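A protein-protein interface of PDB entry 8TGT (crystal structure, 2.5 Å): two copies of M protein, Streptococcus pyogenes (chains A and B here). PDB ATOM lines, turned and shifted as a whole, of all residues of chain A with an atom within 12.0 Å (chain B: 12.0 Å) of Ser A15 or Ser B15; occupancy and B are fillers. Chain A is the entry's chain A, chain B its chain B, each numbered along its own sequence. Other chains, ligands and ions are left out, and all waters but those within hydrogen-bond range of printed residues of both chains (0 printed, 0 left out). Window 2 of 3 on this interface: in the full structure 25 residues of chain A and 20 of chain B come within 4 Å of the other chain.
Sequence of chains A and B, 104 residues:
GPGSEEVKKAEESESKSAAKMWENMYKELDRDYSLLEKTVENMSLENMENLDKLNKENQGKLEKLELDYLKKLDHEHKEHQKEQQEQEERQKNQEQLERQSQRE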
ATOM      1  N   SER A  15     -34.856   2.479 -17.746  1.00  0.00           N
ATOM      2  CA  SER A  15     -33.507   1.994 -17.475  1.00  0.00           C
ATOM      3  C   SER A  15     -32.726   2.999 -16.635  1.00  0.00           C
ATOM      4  O   SER A  15     -31.915   2.615 -15.791  1.00  0.00           O
ATOM      5  CB  SER A  15     -32.763   1.710 -18.782  1.00  0.00           C
ATOM      6  N   LYS A  16     -32.973   4.290 -16.873  1.00  0.00           N
ATOM      7  CA  LYS A  16     -32.310   5.323 -16.084  1.00  0.00           C
ATOM      8  C   LYS A  16     -32.728   5.248 -14.621  1.00  0.00           C
ATOM      9  O   LYS A  16     -31.901   5.432 -13.720  1.00  0.00           O
ATOM     10  CB  LYS A  16     -32.614   6.704 -16.662  1.00  0.00           C
ATOM     11  N   SER A  17     -34.009   4.978 -14.364  1.00  0.00           N
ATOM     12  CA  SER A  17     -34.461   4.800 -12.989  1.00  0.00           C
ATOM     13  C   SER A  17     -33.927   3.507 -12.387  1.00  0.00           C
ATOM     14  O   SER A  17     -33.704   3.435 -11.173  1.00  0.00           O
ATOM     15  CB  SER A  17     -35.988   4.822 -12.932  1.00  0.00           C
ATOM     16  OG  SER A  17     -36.539   3.822 -13.770  1.00  0.00           O
ATOM     17  N   ALA A  18     -33.712   2.483 -13.216  1.00  0.00           N
ATOM     18  CA  ALA A  18     -33.164   1.228 -12.715  1.00  0.00           C
ATOM     19  C   ALA A  18     -31.696   1.378 -12.338  1.00  0.00           C
ATOM     20  O   ALA A  18     -31.233   0.772 -11.365  1.00  0.00           O
ATOM     21  CB  ALA A  18     -33.340   0.126 -13.759  1.00  0.00           C
ATOM     22  N   ALA A  19     -30.949   2.181 -13.099  1.00  0.00           N
ATOM     23  CA  ALA A  19     -29.538   2.386 -12.793  1.00  0.00           C
ATOM     24  C   ALA A  19     -29.351   3.239 -11.546  1.00  0.00           C
ATOM     25  O   ALA A  19     -28.399   3.024 -10.787  1.00  0.00           O
ATOM     26  CB  ALA A  19     -28.830   3.026 -13.987  1.00  0.00           C
ATOM     27  N   LYS A  20     -30.242   4.207 -11.316  1.00  0.00           N
ATOM     28  CA  LYS A  20     -30.123   5.048 -10.130  1.00  0.00           C
ATOM     29  C   LYS A  20     -30.504   4.292  -8.864  1.00  0.00           C
ATOM     30  O   LYS A  20     -29.956   4.566  -7.791  1.00  0.00           O
ATOM     31  CB  LYS A  20     -30.988   6.299 -10.281  1.00  0.00           C
ATOM     32  N   MET A  21     -31.432   3.347  -8.967  1.00  0.00           N
ATOM     33  CA  MET A  21     -31.842   2.556  -7.815  1.00  0.00           C
ATOM     34  C   MET A  21     -30.724   1.629  -7.355  1.00  0.00           C
ATOM     35  O   MET A  21     -30.440   1.528  -6.162  1.00  0.00           O
ATOM     36  CB  MET A  21     -33.091   1.742  -8.138  1.00  0.00           C
ATOM     37  CG  MET A  21     -33.723   1.090  -6.923  1.00  0.00           C
ATOM     38  SD  MET A  21     -34.873  -0.407  -7.398  1.00  0.00           S
ATOM     39  CE  MET A  21     -33.674  -1.346  -8.614  1.00  0.00           C
ATOM     40  N   TRP A  22     -30.093   0.949  -8.315  1.00  0.00           N
ATOM     41  CA  TRP A  22     -29.010   0.034  -7.975  1.00  0.00           C
ATOM     42  C   TRP A  22     -27.758   0.785  -7.545  1.00  0.00           C
ATOM     43  O   TRP A  22     -26.954   0.253  -6.772  1.00  0.00           O
ATOM     44  CB  TRP A  22     -28.712  -0.886  -9.156  1.00  0.00           C
ATOM     45  CG  TRP A  22     -29.627  -2.062  -9.208  1.00  0.00           C
ATOM     46  CD1 TRP A  22     -30.622  -2.287 -10.113  1.00  0.00           C
ATOM     47  CD2 TRP A  22     -29.647  -3.174  -8.305  1.00  0.00           C
ATOM     48  NE1 TRP A  22     -31.257  -3.473  -9.833  1.00  0.00           N
ATOM     49  CE2 TRP A  22     -30.678  -4.036  -8.727  1.00  0.00           C
ATOM     50  CE3 TRP A  22     -28.890  -3.525  -7.184  1.00  0.00           C
ATOM     51  CZ2 TRP A  22     -30.971  -5.228  -8.069  1.00  0.00           C
ATOM     52  CZ3 TRP A  22     -29.185  -4.707  -6.529  1.00  0.00           C
ATOM     53  CH2 TRP A  22     -30.215  -5.544  -6.974  1.00  0.00           C
ATOM     54  N   GLU A  23     -27.573   2.014  -8.031  1.00  0.00           N
ATOM     55  CA  GLU A  23     -26.481   2.842  -7.533  1.00  0.00           C
ATOM     56  C   GLU A  23     -26.739   3.278  -6.097  1.00  0.00           C
ATOM     57  O   GLU A  23     -25.832   3.240  -5.256  1.00  0.00           O
ATOM     58  CB  GLU A  23     -26.286   4.059  -8.438  1.00  0.00           C
ATOM     59  CG  GLU A  23     -25.700   5.271  -7.728  1.00  0.00           C
ATOM     60  CD  GLU A  23     -25.025   6.239  -8.677  1.00  0.00           C
ATOM     61  OE1 GLU A  23     -24.875   5.899  -9.869  1.00  0.00           O
ATOM     62  OE2 GLU A  23     -24.632   7.337  -8.228  1.00  0.00           O
ATOM     63  N   ASN A  24     -27.974   3.686  -5.795  1.00  0.00           N
ATOM     64  CA  ASN A  24     -28.302   4.117  -4.441  1.00  0.00           C
ATOM     65  C   ASN A  24     -28.324   2.947  -3.466  1.00  0.00           C
ATOM     66  O   ASN A  24     -28.094   3.138  -2.267  1.00  0.00           O
ATOM     67  CB  ASN A  24     -29.649   4.839  -4.430  1.00  0.00           C
ATOM     68  N   MET A  25     -28.592   1.741  -3.955  1.00  0.00           N
ATOM     69  CA  MET A  25     -28.637   0.568  -3.094  1.00  0.00           C
ATOM     70  C   MET A  25     -27.239   0.013  -2.845  1.00  0.00           C
ATOM     71  O   MET A  25     -26.975  -0.574  -1.795  1.00  0.00           O
ATOM     72  CB  MET A  25     -29.544  -0.506  -3.694  1.00  0.00           C
ATOM     73  CG  MET A  25     -30.925  -0.543  -3.057  1.00  0.00           C
ATOM     74  SD  MET A  25     -32.038  -2.030  -3.641  1.00  0.00           S
ATOM     75  CE  MET A  25     -31.547  -2.070  -5.524  1.00  0.00           C
ATOM     76  N   GLU B   6     -30.023  10.116 -32.751  1.00  0.00           N
ATOM     77  CA  GLU B   6     -29.329   8.909 -32.320  1.00  0.00           C
ATOM     78  C   GLU B   6     -28.825   9.000 -30.887  1.00  0.00           C
ATOM     79  O   GLU B   6     -28.323   7.999 -30.361  1.00  0.00           O
ATOM     80  CB  GLU B   6     -28.159   8.612 -33.260  1.00  0.00           C
ATOM     81  N   VAL B   7     -28.940  10.166 -30.248  1.00  0.00           N
ATOM     82  CA  VAL B   7     -28.516  10.295 -28.857  1.00  0.00           C
ATOM     83  C   VAL B   7     -29.395   9.444 -27.954  1.00  0.00           C
ATOM     84  O   VAL B   7     -28.899   8.747 -27.062  1.00  0.00           O
ATOM     85  CB  VAL B   7     -28.528  11.774 -28.426  1.00  0.00           C
ATOM     86  N   LYS B   8     -30.713   9.480 -28.177  1.00  0.00           N
ATOM     87  CA  LYS B   8     -31.634   8.710 -27.347  1.00  0.00           C
ATOM     88  C   LYS B   8     -31.280   7.229 -27.337  1.00  0.00           C
ATOM     89  O   LYS B   8     -31.440   6.560 -26.309  1.00  0.00           O
ATOM     90  CB  LYS B   8     -33.071   8.912 -27.833  1.00  0.00           C
ATOM     91  N   LYS B   9     -30.794   6.700 -28.462  1.00  0.00           N
ATOM     92  CA  LYS B   9     -30.339   5.315 -28.484  1.00  0.00           C
ATOM     93  C   LYS B   9     -29.073   5.132 -27.657  1.00  0.00           C
ATOM     94  O   LYS B   9     -28.830   4.041 -27.131  1.00  0.00           O
ATOM     95  CB  LYS B   9     -30.104   4.859 -29.924  1.00  0.00           C
ATOM     96  N   ALA B  10     -28.260   6.182 -27.530  1.00  0.00           N
ATOM     97  CA  ALA B  10     -27.043   6.093 -26.734  1.00  0.00           C
ATOM     98  C   ALA B  10     -27.320   6.263 -25.247  1.00  0.00           C
ATOM     99  O   ALA B  10     -26.610   5.678 -24.420  1.00  0.00           O
ATOM    100  CB  ALA B  10     -26.028   7.136 -27.205  1.00  0.00           C
ATOM    101  N   GLU B  11     -28.334   7.054 -24.884  1.00  0.00           N
ATOM    102  CA  GLU B  11     -28.681   7.201 -23.475  1.00  0.00           C
ATOM    103  C   GLU B  11     -29.254   5.905 -22.915  1.00  0.00           C
ATOM    104  O   GLU B  11     -28.852   5.451 -21.838  1.00  0.00           O
ATOM    105  CB  GLU B  11     -29.671   8.351 -23.291  1.00  0.00           C
ATOM    106  CG  GLU B  11     -29.402   9.556 -24.166  1.00  0.00           C
ATOM    107  CD  GLU B  11     -30.092  10.806 -23.666  1.00  0.00           C
ATOM    108  OE1 GLU B  11     -29.389  11.749 -23.243  1.00  0.00           O
ATOM    109  OE2 GLU B  11     -31.340  10.845 -23.694  1.00  0.00           O
ATOM    110  N   GLU B  12     -30.198   5.292 -23.635  1.00  0.00           N
ATOM    111  CA  GLU B  12     -30.768   4.029 -23.179  1.00  0.00           C
ATOM    112  C   GLU B  12     -29.723   2.922 -23.150  1.00  0.00           C
ATOM    113  O   GLU B  12     -29.774   2.046 -22.280  1.00  0.00           O
ATOM    114  CB  GLU B  12     -31.944   3.628 -24.072  1.00  0.00           C
ATOM    115  N   SER B  13     -28.772   2.944 -24.086  1.00  0.00           N
ATOM    116  CA  SER B  13     -27.704   1.951 -24.067  1.00  0.00           C
ATOM    117  C   SER B  13     -26.782   2.161 -22.873  1.00  0.00           C
ATOM    118  O   SER B  13     -26.365   1.193 -22.225  1.00  0.00           O
ATOM    119  CB  SER B  13     -26.914   2.004 -25.375  1.00  0.00           C
ATOM    120  OG  SER B  13     -26.000   0.925 -25.462  1.00  0.00           O
ATOM    121  N   GLU B  14     -26.458   3.419 -22.564  1.00  0.00           N
ATOM    122  CA  GLU B  14     -25.612   3.704 -21.410  1.00  0.00           C
ATOM    123  C   GLU B  14     -26.345   3.417 -20.105  1.00  0.00           C
ATOM    124  O   GLU B  14     -25.745   2.911 -19.149  1.00  0.00           O
ATOM    125  CB  GLU B  14     -25.140   5.157 -21.454  1.00  0.00           C
ATOM    126  CG  GLU B  14     -24.180   5.537 -20.336  1.00  0.00           C
ATOM    127  CD  GLU B  14     -24.888   6.129 -19.132  1.00  0.00           C
ATOM    128  OE1 GLU B  14     -25.987   6.697 -19.307  1.00  0.00           O
ATOM    129  OE2 GLU B  14     -24.349   6.019 -18.010  1.00  0.00           O
ATOM    130  N   SER B  15     -27.639   3.737 -20.043  1.00  0.00           N
ATOM    131  CA  SER B  15     -28.405   3.471 -18.829  1.00  0.00           C
ATOM    132  C   SER B  15     -28.556   1.973 -18.588  1.00  0.00           C
ATOM    133  O   SER B  15     -28.536   1.520 -17.438  1.00  0.00           O
ATOM    134  CB  SER B  15     -29.774   4.143 -18.913  1.00  0.00           C
ATOM    135  OG  SER B  15     -29.710   5.488 -18.472  1.00  0.00           O
ATOM    136  N   LYS B  16     -28.702   1.190 -19.660  1.00  0.00           N
ATOM    137  CA  LYS B  16     -28.843  -0.254 -19.504  1.00  0.00           C
ATOM    138  C   LYS B  16     -27.552  -0.885 -19.000  1.00  0.00           C
ATOM    139  O   LYS B  16     -27.582  -1.748 -18.114  1.00  0.00           O
ATOM    140  CB  LYS B  16     -29.269  -0.885 -20.830  1.00  0.00           C
ATOM    141  N   SER B  17     -26.408  -0.473 -19.550  1.00  0.00           N
ATOM    142  CA  SER B  17     -25.133  -1.003 -19.082  1.00  0.00           C
ATOM    143  C   SER B  17     -24.808  -0.517 -17.677  1.00  0.00           C
ATOM    144  O   SER B  17     -24.182  -1.245 -16.900  1.00  0.00           O
ATOM    145  CB  SER B  17     -24.015  -0.622 -20.050  1.00  0.00           C
ATOM    146  N   ALA B  18     -25.220   0.707 -17.335  1.00  0.00           N
ATOM    147  CA  ALA B  18     -25.027   1.191 -15.972  1.00  0.00           C
ATOM    148  C   ALA B  18     -25.917   0.435 -14.993  1.00  0.00           C
ATOM    149  O   ALA B  18     -25.498   0.134 -13.870  1.00  0.00           O
ATOM    150  CB  ALA B  18     -25.299   2.693 -15.901  1.00  0.00           C
ATOM    151  N   ALA B  19     -27.149   0.119 -15.402  1.00  0.00           N
ATOM    152  CA  ALA B  19     -28.031  -0.668 -14.546  1.00  0.00           C
ATOM    153  C   ALA B  19     -27.473  -2.068 -14.325  1.00  0.00           C
ATOM    154  O   ALA B  19     -27.536  -2.601 -13.212  1.00  0.00           O
ATOM    155  CB  ALA B  19     -29.432  -0.736 -15.153  1.00  0.00           C
ATOM    156  N   LYS B  20     -26.920  -2.679 -15.375  1.00  0.00           N
ATOM    157  CA  LYS B  20     -26.275  -3.978 -15.233  1.00  0.00           C
ATOM    158  C   LYS B  20     -24.951  -3.892 -14.486  1.00  0.00           C
ATOM    159  O   LYS B  20     -24.404  -4.934 -14.106  1.00  0.00           O
ATOM    160  CB  LYS B  20     -26.053  -4.610 -16.609  1.00  0.00           C
ATOM    161  N   MET B  21     -24.427  -2.691 -14.270  1.00  0.00           N
ATOM    162  CA  MET B  21     -23.193  -2.517 -13.520  1.00  0.00           C
ATOM    163  C   MET B  21     -23.480  -2.416 -12.026  1.00  0.00           C
ATOM    164  O   MET B  21     -23.047  -3.267 -11.253  1.00  0.00           O
ATOM    165  CB  MET B  21     -22.442  -1.275 -14.002  1.00  0.00           C
ATOM    166  CG  MET B  21     -20.931  -1.382 -13.874  1.00  0.00           C
ATOM    167  SD  MET B  21     -20.039   0.352 -13.869  1.00  0.00           S
ATOM    168  CE  MET B  21     -21.204   1.295 -12.616  1.00  0.00           C
ATOM    169  N   TRP B  22     -24.227  -1.379 -11.632  1.00  0.00           N
ATOM    170  CA  TRP B  22     -24.545  -1.167 -10.223  1.00  0.00           C
ATOM    171  C   TRP B  22     -25.276  -2.354  -9.604  1.00  0.00           C
ATOM    172  O   TRP B  22     -25.216  -2.535  -8.384  1.00  0.00           O
ATOM    173  CB  TRP B  22     -25.380   0.104 -10.055  1.00  0.00           C
ATOM    174  CG  TRP B  22     -24.668   1.356 -10.474  1.00  0.00           C
ATOM    175  CD1 TRP B  22     -24.819   2.027 -11.652  1.00  0.00           C
ATOM    176  CD2 TRP B  22     -23.697   2.091  -9.716  1.00  0.00           C
ATOM    177  NE1 TRP B  22     -24.002   3.130 -11.677  1.00  0.00           N
ATOM    178  CE2 TRP B  22     -23.303   3.193 -10.501  1.00  0.00           C
ATOM    179  CE3 TRP B  22     -23.122   1.924  -8.453  1.00  0.00           C
ATOM    180  CZ2 TRP B  22     -22.358   4.121 -10.066  1.00  0.00           C
ATOM    181  CZ3 TRP B  22     -22.187   2.850  -8.021  1.00  0.00           C
ATOM    182  CH2 TRP B  22     -21.815   3.934  -8.826  1.00  0.00           C
ATOM    183  N   GLU B  23     -25.966  -3.161 -10.413  1.00  0.00           N
ATOM    184  CA  GLU B  23     -26.566  -4.386  -9.896  1.00  0.00           C
ATOM    185  C   GLU B  23     -25.520  -5.477  -9.696  1.00  0.00           C
ATOM    186  O   GLU B  23     -25.608  -6.258  -8.742  1.00  0.00           O
ATOM    187  CB  GLU B  23     -27.661  -4.879 -10.842  1.00  0.00           C
ATOM    188  CG  GLU B  23     -28.421  -6.096 -10.332  1.00  0.00           C
ATOM    189  CD  GLU B  23     -29.662  -6.394 -11.152  1.00  0.00           C
ATOM    190  OE1 GLU B  23     -30.463  -5.465 -11.381  1.00  0.00           O
ATOM    191  OE2 GLU B  23     -29.835  -7.559 -11.567  1.00  0.00           O
ATOM    192  N   ASN B  24     -24.524  -5.540 -10.582  1.00  0.00           N
ATOM    193  CA  ASN B  24     -23.550  -6.624 -10.522  1.00  0.00           C
ATOM    194  C   ASN B  24     -22.593  -6.453  -9.348  1.00  0.00           C
ATOM    195  O   ASN B  24     -22.272  -7.429  -8.659  1.00  0.00           O
ATOM    196  CB  ASN B  24     -22.785  -6.712 -11.842  1.00  0.00           C
ATOM    197  CG  ASN B  24     -23.408  -7.701 -12.813  1.00  0.00           C
ATOM    198  OD1 ASN B  24     -23.819  -8.795 -12.424  1.00  0.00           O
ATOM    199  ND2 ASN B  24     -23.485  -7.316 -14.082  1.00  0.00           N
ATOM    200  N   MET B  25     -22.130  -5.232  -9.098  1.00  0.00           N
ATOM    201  CA  MET B  25     -21.216  -5.002  -7.985  1.00  0.00           C
ATOM    202  C   MET B  25     -21.978  -5.039  -6.659  1.00  0.00           C
ATOM    203  O   MET B  25     -21.386  -5.248  -5.599  1.00  0.00           O
ATOM    204  CB  MET B  25     -20.465  -3.675  -8.150  1.00  0.00           C
ATOM    205  CG  MET B  25     -21.218  -2.600  -8.909  1.00  0.00           C
ATOM    206  SD  MET B  25     -20.089  -1.084  -9.419  1.00  0.00           S
ATOM    207  CE  MET B  25     -20.256  -0.034  -7.789  1.00  0.00           C
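The side-chain carboxylate (OE1) of Glu B23 is in hydrogen-bond range of the indole nitrogen (NE1) of Trp A22, at 2.6 Å.
The indole nitrogen (NE1) of Trp B22 sits close to the side-chain carboxylate (OE1) of Glu A23, 3.4 Å away.
O of Glu B11 sits close to OG of Ser B15 (3.5 Å).
Ser A15 touches Ser B15.
Lys A16 touches Ser B15.
Ala A19 touches Ser B15 (CB to O, 3.8 Å).
CB of Ala A19 touches N of Ala B19, 3.6 Å away.
Ala A19 touches Trp B22.
Trp A22 touches Trp B22.
Printed residues of chain A within 4 Å of Ser B15: Ser A15 (3.9 Å), Lys A16 (3.5 Å) and Ala A19 (3.8 Å).
Lys A16 touches just one residue of chain B: Ser B15 (3.5 Å).
Ser A17 touches none of the printed residues of chain B.
No residue of chain B comes within 4 Å of Ala A18.
Ala A19 touches just these residues of chain B: Ser B15, Ala B19 and Trp B22.
No residue of chain A comes within 4 Å of Glu B12.
No residue of chain A comes within 4 Å of Ser B13.
No residue of chain A comes within 4 Å of Lys B16.
No residue of chain A comes within 4 Å of Ser B17.
Ala B18 touches none of the printed residues of chain A.
Ala B19 touches one residue of chain A.
Of the printed residues of chain A, Glu B23 touches Trp A22 (2.6 Å).
Printed residues of chain B within 4 Å of Trp A22: Trp B22 and Glu B23.
Asn A24 touches none of the printed residues of chain B.
Met A21 touches none of the printed residues of chain B.
The nearest residue of chain B that does not touch Ser A15 is Lys B16 (4.2 Å).
The nearest residue of chain A that does not touch Ser B15 is Ser A17 (6.0 Å).
The nearest printed residue of chain B that does not touch Trp A22 is Ala B19 (4.4 Å).
Hydrophobic or aromatic side chains of chain B that line the printed part of chain A: Ala B19 and Trp B22.
Along chain B the printed residues that touch a printed residue of chain A span positions 15 to 23.
Of the 11 printed residues of chain A, 5 touch a printed residue of chain B.
Printed residues of chain A that touch a printed residue of chain B: Ser A15, Lys A16, Ala A19, Trp A22 and Glu A23.
Among the printed residues, no Asp or Glu carboxylate lies within 4 Å of a Lys or Arg side-chain nitrogen of the other chain.
Ser B15 touches its own counterpart, Ser A15.
Lys A16 touches Ser B15, but with the chains exchanged Ser A15 does not touch Lys B16 (4.2 Å).
Trp A22 touches its own counterpart, Trp B22.
Trp A22 touches Glu B23, and with the chains exchanged Glu A23 touches Trp B22.
Positions printed for both chains: 15, 16, 17, 18, 19, 20, 21, 22, 23, 24 and 25.
Of the 8 pairs that touch across the chains among the printed residues, 5 have their exchanged pair printed and touching as well.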
